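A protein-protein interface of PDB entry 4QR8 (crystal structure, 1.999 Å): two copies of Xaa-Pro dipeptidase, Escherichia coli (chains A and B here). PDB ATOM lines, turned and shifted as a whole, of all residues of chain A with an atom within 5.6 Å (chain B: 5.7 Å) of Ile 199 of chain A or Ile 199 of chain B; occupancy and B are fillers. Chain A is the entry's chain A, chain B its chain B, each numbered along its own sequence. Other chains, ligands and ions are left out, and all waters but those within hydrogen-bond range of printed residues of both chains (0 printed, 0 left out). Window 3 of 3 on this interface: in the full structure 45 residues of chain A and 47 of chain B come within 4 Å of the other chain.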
ATOM      1  N   GLU A 194       4.927 -14.487  -0.921  1.00  0.00           N
ATOM      2  CA  GLU A 194       4.069 -13.489  -0.287  1.00  0.00           C
ATOM      3  C   GLU A 194       2.592 -13.884  -0.380  1.00  0.00           C
ATOM      4  O   GLU A 194       1.846 -13.745   0.587  1.00  0.00           O
ATOM      5  CB  GLU A 194       4.307 -12.106  -0.912  1.00  0.00           C
ATOM      6  CG  GLU A 194       5.721 -11.573  -0.687  1.00  0.00           C
ATOM      7  CD  GLU A 194       6.009 -10.291  -1.448  1.00  0.00           C
ATOM      8  OE1 GLU A 194       5.303 -10.010  -2.438  1.00  0.00           O
ATOM      9  OE2 GLU A 194       6.948  -9.566  -1.053  1.00  0.00           O
ATOM     10  N   PHE A 195       2.184 -14.398  -1.537  1.00  0.00           N
ATOM     11  CA  PHE A 195       0.805 -14.844  -1.745  1.00  0.00           C
ATOM     12  C   PHE A 195       0.402 -15.958  -0.761  1.00  0.00           C
ATOM     13  O   PHE A 195      -0.677 -15.920  -0.143  1.00  0.00           O
ATOM     14  CB  PHE A 195       0.632 -15.308  -3.196  1.00  0.00           C
ATOM     15  CG  PHE A 195      -0.781 -15.679  -3.558  1.00  0.00           C
ATOM     16  CD1 PHE A 195      -1.679 -14.710  -3.978  1.00  0.00           C
ATOM     17  CD2 PHE A 195      -1.209 -16.998  -3.490  1.00  0.00           C
ATOM     18  CE1 PHE A 195      -2.982 -15.047  -4.315  1.00  0.00           C
ATOM     19  CE2 PHE A 195      -2.513 -17.341  -3.826  1.00  0.00           C
ATOM     20  CZ  PHE A 195      -3.400 -16.363  -4.239  1.00  0.00           C
ATOM     21  N   ASP A 196       1.280 -16.945  -0.612  1.00  0.00           N
ATOM     22  CA  ASP A 196       1.007 -18.079   0.263  1.00  0.00           C
ATOM     23  C   ASP A 196       1.078 -17.684   1.736  1.00  0.00           C
ATOM     24  O   ASP A 196       0.304 -18.180   2.559  1.00  0.00           O
ATOM     25  CB  ASP A 196       1.957 -19.239  -0.044  1.00  0.00           C
ATOM     26  CG  ASP A 196       1.653 -19.900  -1.378  1.00  0.00           C
ATOM     27  OD1 ASP A 196       0.459 -20.076  -1.701  1.00  0.00           O
ATOM     28  OD2 ASP A 196       2.609 -20.237  -2.110  1.00  0.00           O
ATOM     29  N   ILE A 197       2.001 -16.783   2.062  1.00  0.00           N
ATOM     30  CA  ILE A 197       2.085 -16.244   3.414  1.00  0.00           C
ATOM     31  C   ILE A 197       0.791 -15.516   3.760  1.00  0.00           C
ATOM     32  O   ILE A 197       0.251 -15.668   4.860  1.00  0.00           O
ATOM     33  CB  ILE A 197       3.287 -15.295   3.575  1.00  0.00           C
ATOM     34  CG1 ILE A 197       4.594 -16.083   3.477  1.00  0.00           C
ATOM     35  CG2 ILE A 197       3.220 -14.569   4.913  1.00  0.00           C
ATOM     36  CD1 ILE A 197       5.834 -15.213   3.393  1.00  0.00           C
ATOM     37  N   ASN A 198       0.286 -14.739   2.807  1.00  0.00           N
ATOM     38  CA  ASN A 198      -0.981 -14.052   2.999  1.00  0.00           C
ATOM     39  C   ASN A 198      -2.103 -15.047   3.263  1.00  0.00           C
ATOM     40  O   ASN A 198      -2.877 -14.877   4.209  1.00  0.00           O
ATOM     41  CB  ASN A 198      -1.317 -13.167   1.801  1.00  0.00           C
ATOM     42  CG  ASN A 198      -2.480 -12.237   2.081  1.00  0.00           C
ATOM     43  OD1 ASN A 198      -2.408 -11.390   2.976  1.00  0.00           O
ATOM     44  ND2 ASN A 198      -3.562 -12.386   1.317  1.00  0.00           N
ATOM     45  N   ILE A 199      -2.173 -16.090   2.435  1.00  0.00           N
ATOM     46  CA  ILE A 199      -3.123 -17.179   2.663  1.00  0.00           C
ATOM     47  C   ILE A 199      -3.042 -17.734   4.090  1.00  0.00           C
ATOM     48  O   ILE A 199      -4.067 -17.929   4.748  1.00  0.00           O
ATOM     49  CB  ILE A 199      -2.914 -18.338   1.666  1.00  0.00           C
ATOM     50  CG1 ILE A 199      -3.331 -17.915   0.254  1.00  0.00           C
ATOM     51  CG2 ILE A 199      -3.695 -19.575   2.110  1.00  0.00           C
ATOM     52  CD1 ILE A 199      -4.783 -17.548   0.137  1.00  0.00           C
ATOM     53  N   ALA A 200      -1.824 -17.979   4.566  1.00  0.00           N
ATOM     54  CA  ALA A 200      -1.630 -18.512   5.911  1.00  0.00           C
ATOM     55  C   ALA A 200      -2.147 -17.540   6.971  1.00  0.00           C
ATOM     56  O   ALA A 200      -2.782 -17.950   7.951  1.00  0.00           O
ATOM     57  CB  ALA A 200      -0.165 -18.842   6.148  1.00  0.00           C
ATOM     58  N   TYR A 201      -1.890 -16.251   6.762  1.00  0.00           N
ATOM     59  CA  TYR A 201      -2.374 -15.226   7.684  1.00  0.00           C
ATOM     60  C   TYR A 201      -3.901 -15.219   7.754  1.00  0.00           C
ATOM     61  O   TYR A 201      -4.486 -15.224   8.844  1.00  0.00           O
ATOM     62  CB  TYR A 201      -1.855 -13.837   7.299  1.00  0.00           C
ATOM     63  CG  TYR A 201      -2.210 -12.767   8.312  1.00  0.00           C
ATOM     64  CD1 TYR A 201      -1.360 -12.474   9.369  1.00  0.00           C
ATOM     65  CD2 TYR A 201      -3.404 -12.063   8.219  1.00  0.00           C
ATOM     66  CE1 TYR A 201      -1.688 -11.504  10.302  1.00  0.00           C
ATOM     67  CE2 TYR A 201      -3.738 -11.095   9.144  1.00  0.00           C
ATOM     68  CZ  TYR A 201      -2.879 -10.820  10.185  1.00  0.00           C
ATOM     69  OH  TYR A 201      -3.213  -9.851  11.102  1.00  0.00           O
ATOM     70  N   LEU A 202      -4.540 -15.213   6.587  1.00  0.00           N
ATOM     71  CA  LEU A 202      -5.998 -15.208   6.511  1.00  0.00           C
ATOM     72  C   LEU A 202      -6.602 -16.455   7.150  1.00  0.00           C
ATOM     73  O   LEU A 202      -7.620 -16.376   7.843  1.00  0.00           O
ATOM     74  CB  LEU A 202      -6.462 -15.082   5.056  1.00  0.00           C
ATOM     75  CG  LEU A 202      -6.116 -13.779   4.329  1.00  0.00           C
ATOM     76  CD1 LEU A 202      -6.544 -13.851   2.870  1.00  0.00           C
ATOM     77  CD2 LEU A 202      -6.765 -12.589   5.017  1.00  0.00           C
ATOM     78  N   THR A 203      -5.975 -17.604   6.906  1.00  0.00           N
ATOM     79  CA  THR A 203      -6.433 -18.862   7.484  1.00  0.00           C
ATOM     80  C   THR A 203      -6.358 -18.817   9.005  1.00  0.00           C
ATOM     81  O   THR A 203      -7.291 -19.229   9.693  1.00  0.00           O
ATOM     82  CB  THR A 203      -5.623 -20.063   6.962  1.00  0.00           C
ATOM     83  OG1 THR A 203      -5.875 -20.236   5.563  1.00  0.00           O
ATOM     84  CG2 THR A 203      -6.024 -21.336   7.693  1.00  0.00           C
ATOM     85  N   ALA A 204      -5.253 -18.296   9.527  1.00  0.00           N
ATOM     86  CA  ALA A 204      -5.080 -18.218  10.973  1.00  0.00           C
ATOM     87  C   ALA A 204      -6.036 -17.224  11.628  1.00  0.00           C
ATOM     88  O   ALA A 204      -6.508 -17.460  12.741  1.00  0.00           O
ATOM     89  CB  ALA A 204      -3.644 -17.885  11.324  1.00  0.00           C
ATOM     90  N   GLU B 194     -16.890 -24.193   3.964  1.00  0.00           N
ATOM     91  CA  GLU B 194     -16.977 -23.255   2.849  1.00  0.00           C
ATOM     92  C   GLU B 194     -15.760 -22.328   2.817  1.00  0.00           C
ATOM     93  O   GLU B 194     -15.239 -22.008   1.749  1.00  0.00           O
ATOM     94  CB  GLU B 194     -18.271 -22.436   2.934  1.00  0.00           C
ATOM     95  CG  GLU B 194     -19.541 -23.268   2.845  1.00  0.00           C
ATOM     96  CD  GLU B 194     -20.800 -22.457   3.107  1.00  0.00           C
ATOM     97  OE1 GLU B 194     -20.708 -21.407   3.777  1.00  0.00           O
ATOM     98  OE2 GLU B 194     -21.883 -22.876   2.644  1.00  0.00           O
ATOM     99  N   PHE B 195     -15.310 -21.910   3.996  1.00  0.00           N
ATOM    100  CA  PHE B 195     -14.184 -20.987   4.115  1.00  0.00           C
ATOM    101  C   PHE B 195     -12.888 -21.604   3.586  1.00  0.00           C
ATOM    102  O   PHE B 195     -12.126 -20.962   2.850  1.00  0.00           O
ATOM    103  CB  PHE B 195     -14.018 -20.562   5.574  1.00  0.00           C
ATOM    104  CG  PHE B 195     -12.941 -19.541   5.793  1.00  0.00           C
ATOM    105  CD1 PHE B 195     -13.178 -18.201   5.535  1.00  0.00           C
ATOM    106  CD2 PHE B 195     -11.695 -19.918   6.271  1.00  0.00           C
ATOM    107  CE1 PHE B 195     -12.189 -17.254   5.743  1.00  0.00           C
ATOM    108  CE2 PHE B 195     -10.701 -18.976   6.479  1.00  0.00           C
ATOM    109  CZ  PHE B 195     -10.949 -17.643   6.214  1.00  0.00           C
ATOM    110  N   ASP B 196     -12.647 -22.856   3.965  1.00  0.00           N
ATOM    111  CA  ASP B 196     -11.459 -23.576   3.526  1.00  0.00           C
ATOM    112  C   ASP B 196     -11.521 -23.919   2.035  1.00  0.00           C
ATOM    113  O   ASP B 196     -10.504 -23.886   1.339  1.00  0.00           O
ATOM    114  CB  ASP B 196     -11.247 -24.829   4.374  1.00  0.00           C
ATOM    115  CG  ASP B 196     -10.873 -24.502   5.812  1.00  0.00           C
ATOM    116  OD1 ASP B 196     -10.049 -23.585   6.020  1.00  0.00           O
ATOM    117  OD2 ASP B 196     -11.406 -25.152   6.735  1.00  0.00           O
ATOM    118  N   ILE B 197     -12.716 -24.243   1.550  1.00  0.00           N
ATOM    119  CA  ILE B 197     -12.918 -24.484   0.124  1.00  0.00           C
ATOM    120  C   ILE B 197     -12.596 -23.225  -0.667  1.00  0.00           C
ATOM    121  O   ILE B 197     -11.922 -23.283  -1.700  1.00  0.00           O
ATOM    122  CB  ILE B 197     -14.361 -24.928  -0.186  1.00  0.00           C
ATOM    123  CG1 ILE B 197     -14.636 -26.302   0.427  1.00  0.00           C
ATOM    124  CG2 ILE B 197     -14.595 -24.976  -1.691  1.00  0.00           C
ATOM    125  CD1 ILE B 197     -16.091 -26.705   0.388  1.00  0.00           C
ATOM    126  N   ASN B 198     -13.063 -22.085  -0.166  1.00  0.00           N
ATOM    127  CA  ASN B 198     -12.753 -20.806  -0.789  1.00  0.00           C
ATOM    128  C   ASN B 198     -11.245 -20.559  -0.802  1.00  0.00           C
ATOM    129  O   ASN B 198     -10.686 -20.098  -1.807  1.00  0.00           O
ATOM    130  CB  ASN B 198     -13.481 -19.660  -0.083  1.00  0.00           C
ATOM    131  CG  ASN B 198     -13.338 -18.340  -0.822  1.00  0.00           C
ATOM    132  OD1 ASN B 198     -13.865 -18.175  -1.923  1.00  0.00           O
ATOM    133  ND2 ASN B 198     -12.625 -17.394  -0.221  1.00  0.00           N
ATOM    134  N   ILE B 199     -10.588 -20.882   0.310  1.00  0.00           N
ATOM    135  CA  ILE B 199      -9.128 -20.792   0.368  1.00  0.00           C
ATOM    136  C   ILE B 199      -8.496 -21.621  -0.753  1.00  0.00           C
ATOM    137  O   ILE B 199      -7.608 -21.147  -1.462  1.00  0.00           O
ATOM    138  CB  ILE B 199      -8.565 -21.264   1.725  1.00  0.00           C
ATOM    139  CG1 ILE B 199      -8.976 -20.309   2.847  1.00  0.00           C
ATOM    140  CG2 ILE B 199      -7.050 -21.380   1.663  1.00  0.00           C
ATOM    141  CD1 ILE B 199      -8.414 -18.918   2.700  1.00  0.00           C
ATOM    142  N   ALA B 200      -8.971 -22.852  -0.914  1.00  0.00           N
ATOM    143  CA  ALA B 200      -8.458 -23.746  -1.954  1.00  0.00           C
ATOM    144  C   ALA B 200      -8.648 -23.171  -3.363  1.00  0.00           C
ATOM    145  O   ALA B 200      -7.752 -23.264  -4.218  1.00  0.00           O
ATOM    146  CB  ALA B 200      -9.119 -25.108  -1.846  1.00  0.00           C
ATOM    147  N   TYR B 201      -9.814 -22.575  -3.597  1.00  0.00           N
ATOM    148  CA  TYR B 201     -10.114 -21.962  -4.889  1.00  0.00           C
ATOM    149  C   TYR B 201      -9.163 -20.806  -5.185  1.00  0.00           C
ATOM    150  O   TYR B 201      -8.588 -20.720  -6.279  1.00  0.00           O
ATOM    151  CB  TYR B 201     -11.567 -21.473  -4.941  1.00  0.00           C
ATOM    152  CG  TYR B 201     -11.981 -21.026  -6.323  1.00  0.00           C
ATOM    153  CD1 TYR B 201     -12.464 -21.940  -7.247  1.00  0.00           C
ATOM    154  CD2 TYR B 201     -11.860 -19.700  -6.715  1.00  0.00           C
ATOM    155  CE1 TYR B 201     -12.828 -21.549  -8.515  1.00  0.00           C
ATOM    156  CE2 TYR B 201     -12.222 -19.295  -7.985  1.00  0.00           C
ATOM    157  CZ  TYR B 201     -12.701 -20.225  -8.883  1.00  0.00           C
ATOM    158  OH  TYR B 201     -13.067 -19.838 -10.150  1.00  0.00           O
ATOM    159  N   LEU B 202      -8.998 -19.927  -4.197  1.00  0.00           N
ATOM    160  CA  LEU B 202      -8.133 -18.760  -4.332  1.00  0.00           C
ATOM    161  C   LEU B 202      -6.685 -19.175  -4.551  1.00  0.00           C
ATOM    162  O   LEU B 202      -5.952 -18.540  -5.312  1.00  0.00           O
ATOM    163  CB  LEU B 202      -8.238 -17.864  -3.094  1.00  0.00           C
ATOM    164  CG  LEU B 202      -9.567 -17.138  -2.881  1.00  0.00           C
ATOM    165  CD1 LEU B 202      -9.556 -16.392  -1.552  1.00  0.00           C
ATOM    166  CD2 LEU B 202      -9.847 -16.182  -4.036  1.00  0.00           C
ATOM    167  N   THR B 203      -6.282 -20.250  -3.881  1.00  0.00           N
ATOM    168  CA  THR B 203      -4.935 -20.784  -4.021  1.00  0.00           C
ATOM    169  C   THR B 203      -4.694 -21.325  -5.428  1.00  0.00           C
ATOM    170  O   THR B 203      -3.661 -21.045  -6.036  1.00  0.00           O
ATOM    171  CB  THR B 203      -4.658 -21.890  -2.986  1.00  0.00           C
ATOM    172  OG1 THR B 203      -4.827 -21.359  -1.665  1.00  0.00           O
ATOM    173  CG2 THR B 203      -3.238 -22.423  -3.132  1.00  0.00           C
ATOM    174  N   ALA B 204      -5.648 -22.091  -5.951  1.00  0.00           N
ATOM    175  CA  ALA B 204      -5.476 -22.683  -7.278  1.00  0.00           C
ATOM    176  C   ALA B 204      -5.564 -21.665  -8.422  1.00  0.00           C
ATOM    177  O   ALA B 204      -4.901 -21.822  -9.452  1.00  0.00           O
ATOM    178  CB  ALA B 204      -6.458 -23.823  -7.496  1.00  0.00           C
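Ile 199 of chain A touches just one residue of chain B: Ile 199 (3.8 Å). Ile 199 of chain B touches just one residue of chain A: Ile 199 (3.8 Å). Of the printed residues of chain A, Phe 195 of chain B touches Leu 202 (3.9 Å). Printed residues of chain B within 4 Å of Phe 195 of chain A: Leu 202. Of the printed residues of chain B, Leu 202 of chain A touches Phe 195. Printed residues of chain A within 4 Å of Leu 202 of chain B: Phe 195. Asp 196 of chain B touches none of the printed residues of chain A. Glu 194 of chain B touches none of the printed residues of chain A. The nearest residue of chain A that does not touch Ile 199 of chain B is Thr 203 of chain A (4.05 Å). The nearest printed residue of chain A that does not touch Leu 202 of chain B is Ile 199 of chain A (4.7 Å).
Phe 195 of chain A touches Leu 202 of chain B, and with the chains exchanged Leu 202 of chain A touches Phe 195 of chain B. Ile 199 of chain B touches its own counterpart, Ile 199 of chain A. Of the 3 pairs that touch across the chains among the printed residues, 3 have their exchanged pair printed and touching as well.
The backbone carbonyl oxygen (O) of Ile 199 of chain A sits at hydrogen-bond distance from the side-chain hydroxyl (OG1) of Thr 203 of chain A (3.0 Å). O of Ile 199 of chain B sits at hydrogen-bond distance from OG1 of Thr 203 of chain B (2.8 Å).
Among the printed residues, pairs that only touch across the chains: Phe 195 of chain A with Leu 202 of chain B, Ile 199 of chain A with Ile 199 of chain B and Leu 202 of chain A with Phe 195 of chain B.
Of the 11 printed residues of chain B, 3 touch a printed residue of chain A. Of the 11 printed residues of chain A, 3 touch a printed residue of chain B. Printed residues of chain A that touch a printed residue of chain B: Phe 195, Ile 199 and Leu 202. Among the printed residues, 3 pairs touch across the chains. Among the printed residues, no Asp or Glu carboxylate lies within 4 Å of a Lys or Arg side-chain nitrogen of the other chain.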
